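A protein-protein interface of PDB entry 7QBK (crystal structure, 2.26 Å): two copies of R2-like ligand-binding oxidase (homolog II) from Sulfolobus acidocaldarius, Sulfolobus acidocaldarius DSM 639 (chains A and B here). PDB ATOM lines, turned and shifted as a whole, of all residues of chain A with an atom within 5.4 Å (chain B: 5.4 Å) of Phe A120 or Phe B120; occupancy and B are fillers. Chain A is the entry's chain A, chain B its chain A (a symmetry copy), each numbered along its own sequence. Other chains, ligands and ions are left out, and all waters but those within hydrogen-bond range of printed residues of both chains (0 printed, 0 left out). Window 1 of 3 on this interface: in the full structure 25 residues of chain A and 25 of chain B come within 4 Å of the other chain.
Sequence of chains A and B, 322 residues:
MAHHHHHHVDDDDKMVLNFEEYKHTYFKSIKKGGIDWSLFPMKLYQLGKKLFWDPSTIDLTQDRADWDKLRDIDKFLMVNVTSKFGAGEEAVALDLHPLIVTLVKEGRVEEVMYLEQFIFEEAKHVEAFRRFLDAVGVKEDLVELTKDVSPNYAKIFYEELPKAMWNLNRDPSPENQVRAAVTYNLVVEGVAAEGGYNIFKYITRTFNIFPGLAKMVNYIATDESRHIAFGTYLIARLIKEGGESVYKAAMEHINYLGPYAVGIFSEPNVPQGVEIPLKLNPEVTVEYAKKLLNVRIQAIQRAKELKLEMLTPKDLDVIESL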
ATOM      1  N   PHE A  52      -7.694  24.558 -25.446  1.00  0.00           N
ATOM      2  CA  PHE A  52      -8.949  24.326 -26.149  1.00  0.00           C
ATOM      3  C   PHE A  52      -8.702  23.708 -27.519  1.00  0.00           C
ATOM      4  O   PHE A  52      -7.740  24.051 -28.209  1.00  0.00           O
ATOM      5  CB  PHE A  52      -9.728  25.633 -26.309  1.00  0.00           C
ATOM      6  CG  PHE A  52     -11.007  25.483 -27.090  1.00  0.00           C
ATOM      7  CD1 PHE A  52     -12.145  24.974 -26.484  1.00  0.00           C
ATOM      8  CD2 PHE A  52     -11.069  25.846 -28.428  1.00  0.00           C
ATOM      9  CE1 PHE A  52     -13.324  24.835 -27.195  1.00  0.00           C
ATOM     10  CE2 PHE A  52     -12.246  25.707 -29.144  1.00  0.00           C
ATOM     11  CZ  PHE A  52     -13.374  25.202 -28.525  1.00  0.00           C
ATOM     12  N   LEU A 115     -17.815  23.285 -13.995  1.00  0.00           N
ATOM     13  CA  LEU A 115     -18.711  22.227 -14.457  1.00  0.00           C
ATOM     14  C   LEU A 115     -19.363  22.580 -15.787  1.00  0.00           C
ATOM     15  O   LEU A 115     -19.667  21.685 -16.584  1.00  0.00           O
ATOM     16  CB  LEU A 115     -19.774  21.939 -13.398  1.00  0.00           C
ATOM     17  CG  LEU A 115     -19.300  21.105 -12.208  1.00  0.00           C
ATOM     18  CD1 LEU A 115     -20.430  20.850 -11.221  1.00  0.00           C
ATOM     19  CD2 LEU A 115     -18.707  19.795 -12.696  1.00  0.00           C
ATOM     20  N   GLU A 116     -19.594  23.872 -16.043  1.00  0.00           N
ATOM     21  CA  GLU A 116     -20.105  24.290 -17.344  1.00  0.00           C
ATOM     22  C   GLU A 116     -19.082  24.025 -18.440  1.00  0.00           C
ATOM     23  O   GLU A 116     -19.442  23.630 -19.555  1.00  0.00           O
ATOM     24  CB  GLU A 116     -20.495  25.771 -17.306  1.00  0.00           C
ATOM     25  CG  GLU A 116     -21.738  26.089 -16.453  1.00  0.00           C
ATOM     26  CD  GLU A 116     -21.932  27.583 -16.213  1.00  0.00           C
ATOM     27  OE1 GLU A 116     -21.008  28.366 -16.516  1.00  0.00           O
ATOM     28  OE2 GLU A 116     -23.012  27.976 -15.720  1.00  0.00           O
ATOM     29  N   GLN A 117     -17.800  24.236 -18.142  1.00  0.00           N
ATOM     30  CA  GLN A 117     -16.752  23.833 -19.070  1.00  0.00           C
ATOM     31  C   GLN A 117     -16.658  22.317 -19.155  1.00  0.00           C
ATOM     32  O   GLN A 117     -16.471  21.758 -20.241  1.00  0.00           O
ATOM     33  CB  GLN A 117     -15.420  24.435 -18.633  1.00  0.00           C
ATOM     34  CG  GLN A 117     -14.270  24.176 -19.579  1.00  0.00           C
ATOM     35  CD  GLN A 117     -12.974  24.761 -19.068  1.00  0.00           C
ATOM     36  OE1 GLN A 117     -12.290  24.156 -18.246  1.00  0.00           O
ATOM     37  NE2 GLN A 117     -12.636  25.954 -19.541  1.00  0.00           N
ATOM     38  N   PHE A 118     -16.795  21.641 -18.014  1.00  0.00           N
ATOM     39  CA  PHE A 118     -16.771  20.182 -17.981  1.00  0.00           C
ATOM     40  C   PHE A 118     -17.830  19.595 -18.909  1.00  0.00           C
ATOM     41  O   PHE A 118     -17.544  18.701 -19.713  1.00  0.00           O
ATOM     42  CB  PHE A 118     -16.983  19.706 -16.539  1.00  0.00           C
ATOM     43  CG  PHE A 118     -16.935  18.212 -16.367  1.00  0.00           C
ATOM     44  CD1 PHE A 118     -18.018  17.420 -16.718  1.00  0.00           C
ATOM     45  CD2 PHE A 118     -15.823  17.602 -15.820  1.00  0.00           C
ATOM     46  CE1 PHE A 118     -17.976  16.052 -16.557  1.00  0.00           C
ATOM     47  CE2 PHE A 118     -15.784  16.235 -15.651  1.00  0.00           C
ATOM     48  CZ  PHE A 118     -16.858  15.460 -16.024  1.00  0.00           C
ATOM     49  N   ILE A 119     -19.068  20.083 -18.802  1.00  0.00           N
ATOM     50  CA  ILE A 119     -20.172  19.509 -19.566  1.00  0.00           C
ATOM     51  C   ILE A 119     -19.953  19.695 -21.059  1.00  0.00           C
ATOM     52  O   ILE A 119     -20.181  18.773 -21.851  1.00  0.00           O
ATOM     53  CB  ILE A 119     -21.508  20.116 -19.104  1.00  0.00           C
ATOM     54  CG1 ILE A 119     -21.910  19.504 -17.772  1.00  0.00           C
ATOM     55  CG2 ILE A 119     -22.591  19.877 -20.136  1.00  0.00           C
ATOM     56  CD1 ILE A 119     -21.904  18.003 -17.809  1.00  0.00           C
ATOM     57  N   PHE A 120     -19.516  20.887 -21.473  1.00  0.00           N
ATOM     58  CA  PHE A 120     -19.295  21.130 -22.896  1.00  0.00           C
ATOM     59  C   PHE A 120     -18.180  20.248 -23.438  1.00  0.00           C
ATOM     60  O   PHE A 120     -18.284  19.712 -24.548  1.00  0.00           O
ATOM     61  CB  PHE A 120     -18.971  22.603 -23.150  1.00  0.00           C
ATOM     62  CG  PHE A 120     -18.480  22.886 -24.548  1.00  0.00           C
ATOM     63  CD1 PHE A 120     -19.276  22.608 -25.649  1.00  0.00           C
ATOM     64  CD2 PHE A 120     -17.224  23.434 -24.759  1.00  0.00           C
ATOM     65  CE1 PHE A 120     -18.829  22.872 -26.934  1.00  0.00           C
ATOM     66  CE2 PHE A 120     -16.771  23.699 -26.044  1.00  0.00           C
ATOM     67  CZ  PHE A 120     -17.576  23.418 -27.130  1.00  0.00           C
ATOM     68  N   GLU A 121     -17.103  20.089 -22.673  1.00  0.00           N
ATOM     69  CA  GLU A 121     -16.016  19.228 -23.117  1.00  0.00           C
ATOM     70  C   GLU A 121     -16.492  17.789 -23.278  1.00  0.00           C
ATOM     71  O   GLU A 121     -16.120  17.111 -24.242  1.00  0.00           O
ATOM     72  CB  GLU A 121     -14.847  19.330 -22.139  1.00  0.00           C
ATOM     73  CG  GLU A 121     -14.162  20.691 -22.180  1.00  0.00           C
ATOM     74  CD  GLU A 121     -13.141  20.868 -21.080  1.00  0.00           C
ATOM     75  OE1 GLU A 121     -13.143  20.049 -20.136  1.00  0.00           O
ATOM     76  OE2 GLU A 121     -12.341  21.824 -21.154  1.00  0.00           O
ATOM     77  N   GLU A 122     -17.349  17.319 -22.364  1.00  0.00           N
ATOM     78  CA  GLU A 122     -17.930  15.987 -22.504  1.00  0.00           C
ATOM     79  C   GLU A 122     -18.728  15.863 -23.794  1.00  0.00           C
ATOM     80  O   GLU A 122     -18.578  14.885 -24.534  1.00  0.00           O
ATOM     81  CB  GLU A 122     -18.814  15.659 -21.298  1.00  0.00           C
ATOM     82  CG  GLU A 122     -18.053  15.486 -19.994  1.00  0.00           C
ATOM     83  CD  GLU A 122     -16.999  14.401 -20.073  1.00  0.00           C
ATOM     84  OE1 GLU A 122     -17.180  13.458 -20.863  1.00  0.00           O
ATOM     85  OE2 GLU A 122     -15.988  14.488 -19.348  1.00  0.00           O
ATOM     86  N   ALA A 123     -19.598  16.835 -24.075  1.00  0.00           N
ATOM     87  CA  ALA A 123     -20.337  16.786 -25.333  1.00  0.00           C
ATOM     88  C   ALA A 123     -19.399  16.923 -26.520  1.00  0.00           C
ATOM     89  O   ALA A 123     -19.661  16.365 -27.592  1.00  0.00           O
ATOM     90  CB  ALA A 123     -21.411  17.870 -25.363  1.00  0.00           C
ATOM     91  N   LYS A 124     -18.297  17.651 -26.345  1.00  0.00           N
ATOM     92  CA  LYS A 124     -17.277  17.717 -27.381  1.00  0.00           C
ATOM     93  C   LYS A 124     -16.634  16.355 -27.611  1.00  0.00           C
ATOM     94  O   LYS A 124     -16.331  15.996 -28.754  1.00  0.00           O
ATOM     95  CB  LYS A 124     -16.238  18.773 -27.003  1.00  0.00           C
ATOM     96  CG  LYS A 124     -15.280  19.143 -28.109  1.00  0.00           C
ATOM     97  CD  LYS A 124     -14.763  20.572 -27.944  1.00  0.00           C
ATOM     98  CE  LYS A 124     -14.146  20.817 -26.571  1.00  0.00           C
ATOM     99  NZ  LYS A 124     -12.999  19.916 -26.247  1.00  0.00           N
ATOM    100  N   HIS A 125     -16.442  15.574 -26.544  1.00  0.00           N
ATOM    101  CA  HIS A 125     -15.950  14.210 -26.709  1.00  0.00           C
ATOM    102  C   HIS A 125     -16.977  13.339 -27.425  1.00  0.00           C
ATOM    103  O   HIS A 125     -16.610  12.491 -28.246  1.00  0.00           O
ATOM    104  CB  HIS A 125     -15.581  13.612 -25.349  1.00  0.00           C
ATOM    105  CG  HIS A 125     -14.540  14.393 -24.611  1.00  0.00           C
ATOM    106  ND1 HIS A 125     -14.253  14.183 -23.279  1.00  0.00           N
ATOM    107  CD2 HIS A 125     -13.710  15.382 -25.022  1.00  0.00           C
ATOM    108  CE1 HIS A 125     -13.294  15.010 -22.900  1.00  0.00           C
ATOM    109  NE2 HIS A 125     -12.950  15.751 -23.938  1.00  0.00           N
ATOM    110  N   PHE B  52     -16.774  31.244 -33.571  1.00  0.00           N
ATOM    111  CA  PHE B  52     -16.521  30.974 -32.162  1.00  0.00           C
ATOM    112  C   PHE B  52     -15.734  32.109 -31.521  1.00  0.00           C
ATOM    113  O   PHE B  52     -14.842  32.696 -32.137  1.00  0.00           O
ATOM    114  CB  PHE B  52     -15.755  29.661 -31.991  1.00  0.00           C
ATOM    115  CG  PHE B  52     -15.395  29.351 -30.564  1.00  0.00           C
ATOM    116  CD1 PHE B  52     -16.339  28.816 -29.701  1.00  0.00           C
ATOM    117  CD2 PHE B  52     -14.116  29.598 -30.082  1.00  0.00           C
ATOM    118  CE1 PHE B  52     -16.014  28.527 -28.386  1.00  0.00           C
ATOM    119  CE2 PHE B  52     -13.787  29.311 -28.768  1.00  0.00           C
ATOM    120  CZ  PHE B  52     -14.738  28.774 -27.921  1.00  0.00           C
ATOM    121  N   LEU B 115     -28.197  21.722 -29.826  1.00  0.00           N
ATOM    122  CA  LEU B 115     -28.560  22.150 -28.477  1.00  0.00           C
ATOM    123  C   LEU B 115     -27.378  22.062 -27.520  1.00  0.00           C
ATOM    124  O   LEU B 115     -27.293  22.849 -26.570  1.00  0.00           O
ATOM    125  CB  LEU B 115     -29.732  21.318 -27.959  1.00  0.00           C
ATOM    126  CG  LEU B 115     -31.103  21.704 -28.518  1.00  0.00           C
ATOM    127  CD1 LEU B 115     -32.208  20.838 -27.928  1.00  0.00           C
ATOM    128  CD2 LEU B 115     -31.374  23.174 -28.256  1.00  0.00           C
ATOM    129  N   GLU B 116     -26.465  21.113 -27.745  1.00  0.00           N
ATOM    130  CA  GLU B 116     -25.249  21.048 -26.941  1.00  0.00           C
ATOM    131  C   GLU B 116     -24.370  22.266 -27.187  1.00  0.00           C
ATOM    132  O   GLU B 116     -23.749  22.792 -26.257  1.00  0.00           O
ATOM    133  CB  GLU B 116     -24.487  19.753 -27.242  1.00  0.00           C
ATOM    134  CG  GLU B 116     -25.172  18.470 -26.735  1.00  0.00           C
ATOM    135  CD  GLU B 116     -24.537  17.196 -27.286  1.00  0.00           C
ATOM    136  OE1 GLU B 116     -23.711  17.290 -28.218  1.00  0.00           O
ATOM    137  OE2 GLU B 116     -24.866  16.098 -26.786  1.00  0.00           O
ATOM    138  N   GLN B 117     -24.306  22.730 -28.435  1.00  0.00           N
ATOM    139  CA  GLN B 117     -23.636  23.992 -28.718  1.00  0.00           C
ATOM    140  C   GLN B 117     -24.423  25.161 -28.144  1.00  0.00           C
ATOM    141  O   GLN B 117     -23.840  26.105 -27.601  1.00  0.00           O
ATOM    142  CB  GLN B 117     -23.452  24.150 -30.224  1.00  0.00           C
ATOM    143  CG  GLN B 117     -22.672  25.377 -30.639  1.00  0.00           C
ATOM    144  CD  GLN B 117     -22.563  25.495 -32.142  1.00  0.00           C
ATOM    145  OE1 GLN B 117     -23.474  25.987 -32.803  1.00  0.00           O
ATOM    146  NE2 GLN B 117     -21.449  25.030 -32.693  1.00  0.00           N
ATOM    147  N   PHE B 118     -25.751  25.103 -28.253  1.00  0.00           N
ATOM    148  CA  PHE B 118     -26.610  26.144 -27.697  1.00  0.00           C
ATOM    149  C   PHE B 118     -26.351  26.331 -26.205  1.00  0.00           C
ATOM    150  O   PHE B 118     -26.173  27.457 -25.728  1.00  0.00           O
ATOM    151  CB  PHE B 118     -28.077  25.779 -27.955  1.00  0.00           C
ATOM    152  CG  PHE B 118     -29.066  26.802 -27.464  1.00  0.00           C
ATOM    153  CD1 PHE B 118     -29.392  26.888 -26.118  1.00  0.00           C
ATOM    154  CD2 PHE B 118     -29.696  27.653 -28.349  1.00  0.00           C
ATOM    155  CE1 PHE B 118     -30.299  27.823 -25.668  1.00  0.00           C
ATOM    156  CE2 PHE B 118     -30.610  28.582 -27.901  1.00  0.00           C
ATOM    157  CZ  PHE B 118     -30.908  28.670 -26.561  1.00  0.00           C
ATOM    158  N   ILE B 119     -26.336  25.230 -25.450  1.00  0.00           N
ATOM    159  CA  ILE B 119     -26.207  25.316 -23.998  1.00  0.00           C
ATOM    160  C   ILE B 119     -24.863  25.912 -23.605  1.00  0.00           C
ATOM    161  O   ILE B 119     -24.787  26.759 -22.708  1.00  0.00           O
ATOM    162  CB  ILE B 119     -26.423  23.930 -23.363  1.00  0.00           C
ATOM    163  CG1 ILE B 119     -27.907  23.598 -23.366  1.00  0.00           C
ATOM    164  CG2 ILE B 119     -25.884  23.897 -21.949  1.00  0.00           C
ATOM    165  CD1 ILE B 119     -28.736  24.686 -22.749  1.00  0.00           C
ATOM    166  N   PHE B 120     -23.783  25.479 -24.262  1.00  0.00           N
ATOM    167  CA  PHE B 120     -22.464  26.008 -23.925  1.00  0.00           C
ATOM    168  C   PHE B 120     -22.372  27.496 -24.234  1.00  0.00           C
ATOM    169  O   PHE B 120     -21.799  28.266 -23.455  1.00  0.00           O
ATOM    170  CB  PHE B 120     -21.370  25.247 -24.673  1.00  0.00           C
ATOM    171  CG  PHE B 120     -20.008  25.892 -24.580  1.00  0.00           C
ATOM    172  CD1 PHE B 120     -19.394  26.077 -23.351  1.00  0.00           C
ATOM    173  CD2 PHE B 120     -19.343  26.307 -25.723  1.00  0.00           C
ATOM    174  CE1 PHE B 120     -18.142  26.666 -23.264  1.00  0.00           C
ATOM    175  CE2 PHE B 120     -18.089  26.895 -25.643  1.00  0.00           C
ATOM    176  CZ  PHE B 120     -17.490  27.073 -24.411  1.00  0.00           C
ATOM    177  N   GLU B 121     -22.927  27.917 -25.369  1.00  0.00           N
ATOM    178  CA  GLU B 121     -22.905  29.333 -25.707  1.00  0.00           C
ATOM    179  C   GLU B 121     -23.668  30.151 -24.671  1.00  0.00           C
ATOM    180  O   GLU B 121     -23.225  31.237 -24.281  1.00  0.00           O
ATOM    181  CB  GLU B 121     -23.467  29.535 -27.112  1.00  0.00           C
ATOM    182  CG  GLU B 121     -22.556  28.974 -28.197  1.00  0.00           C
ATOM    183  CD  GLU B 121     -23.194  28.987 -29.567  1.00  0.00           C
ATOM    184  OE1 GLU B 121     -24.427  29.190 -29.640  1.00  0.00           O
ATOM    185  OE2 GLU B 121     -22.472  28.795 -30.568  1.00  0.00           O
ATOM    186  N   GLU B 122     -24.798  29.625 -24.184  1.00  0.00           N
ATOM    187  CA  GLU B 122     -25.533  30.299 -23.117  1.00  0.00           C
ATOM    188  C   GLU B 122     -24.678  30.451 -21.867  1.00  0.00           C
ATOM    189  O   GLU B 122     -24.620  31.534 -21.273  1.00  0.00           O
ATOM    190  CB  GLU B 122     -26.820  29.538 -22.790  1.00  0.00           C
ATOM    191  CG  GLU B 122     -27.862  29.571 -23.895  1.00  0.00           C
ATOM    192  CD  GLU B 122     -28.268  30.981 -24.274  1.00  0.00           C
ATOM    193  OE1 GLU B 122     -28.198  31.868 -23.407  1.00  0.00           O
ATOM    194  OE2 GLU B 122     -28.658  31.205 -25.437  1.00  0.00           O
ATOM    195  N   ALA B 123     -24.018  29.372 -21.436  1.00  0.00           N
ATOM    196  CA  ALA B 123     -23.139  29.493 -20.278  1.00  0.00           C
ATOM    197  C   ALA B 123     -21.968  30.413 -20.579  1.00  0.00           C
ATOM    198  O   ALA B 123     -21.460  31.094 -19.680  1.00  0.00           O
ATOM    199  CB  ALA B 123     -22.647  28.117 -19.836  1.00  0.00           C
ATOM    200  N   LYS B 124     -21.533  30.454 -21.838  1.00  0.00           N
ATOM    201  CA  LYS B 124     -20.512  31.411 -22.239  1.00  0.00           C
ATOM    202  C   LYS B 124     -21.015  32.843 -22.108  1.00  0.00           C
ATOM    203  O   LYS B 124     -20.254  33.736 -21.716  1.00  0.00           O
ATOM    204  CB  LYS B 124     -20.063  31.101 -23.668  1.00  0.00           C
ATOM    205  CG  LYS B 124     -18.820  31.834 -24.114  1.00  0.00           C
ATOM    206  CD  LYS B 124     -18.061  31.045 -25.180  1.00  0.00           C
ATOM    207  CE  LYS B 124     -18.939  30.667 -26.369  1.00  0.00           C
ATOM    208  NZ  LYS B 124     -19.552  31.837 -27.069  1.00  0.00           N
ATOM    209  N   HIS B 125     -22.295  33.079 -22.408  1.00  0.00           N
ATOM    210  CA  HIS B 125     -22.874  34.400 -22.183  1.00  0.00           C
ATOM    211  C   HIS B 125     -22.943  34.721 -20.694  1.00  0.00           C
ATOM    212  O   HIS B 125     -22.714  35.867 -20.293  1.00  0.00           O
ATOM    213  CB  HIS B 125     -24.260  34.487 -22.824  1.00  0.00           C
ATOM    214  CG  HIS B 125     -24.259  34.230 -24.299  1.00  0.00           C
ATOM    215  ND1 HIS B 125     -25.411  34.004 -25.019  1.00  0.00           N
ATOM    216  CD2 HIS B 125     -23.240  34.165 -25.190  1.00  0.00           C
ATOM    217  CE1 HIS B 125     -25.106  33.812 -26.290  1.00  0.00           C
ATOM    218  NE2 HIS B 125     -23.794  33.902 -26.420  1.00  0.00           N
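CZ of Phe A52 touches CZ of Phe B52, at 3.9 Å. CB of Ala B123 touches OE1 of Glu A116, at 3.7 Å. CG of Phe B120 touches CG of Phe A120, 3.4 Å away. Ala A123 touches Glu B116.
Printed residues of chain B within 4 Å of Phe A52: Phe B52. Printed residues of chain B within 4 Å of Glu A116: Ala B123. Ile A119 touches none of the printed residues of chain B. Phe A120 touches just one residue of chain B: Phe B120 (3.4 Å). Of the printed residues of chain B, Ala A123 touches Glu B116. Printed residues of chain A within 4 Å of Phe B52: Phe A52 (3.9 Å). Of the printed residues of chain A, Phe B120 touches Phe A120. The nearest residue of chain A that does not touch Phe B120 is Glu A116 (4.5 Å).
Hydrophobic or aromatic side chains of chain A within 4 Å of the printed part of chain B: Phe A52, Phe A120 and Ala A123. Of the 12 printed residues of chain B, 4 touch a printed residue of chain A. Among the printed residues, 4 pairs touch across the chains. Among the printed residues, no Asp or Glu carboxylate lies within 4 Å of a Lys or Arg side-chain nitrogen of the other chain.
Phe B52 touches its own counterpart, Phe A52. Glu A116 touches Ala B123, and with the chains exchanged Ala A123 touches Glu B116. Phe A120 touches its own counterpart, Phe B120. Of the 4 pairs that touch across the chains among the printed residues, 4 have their exchanged pair printed and touching as well.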
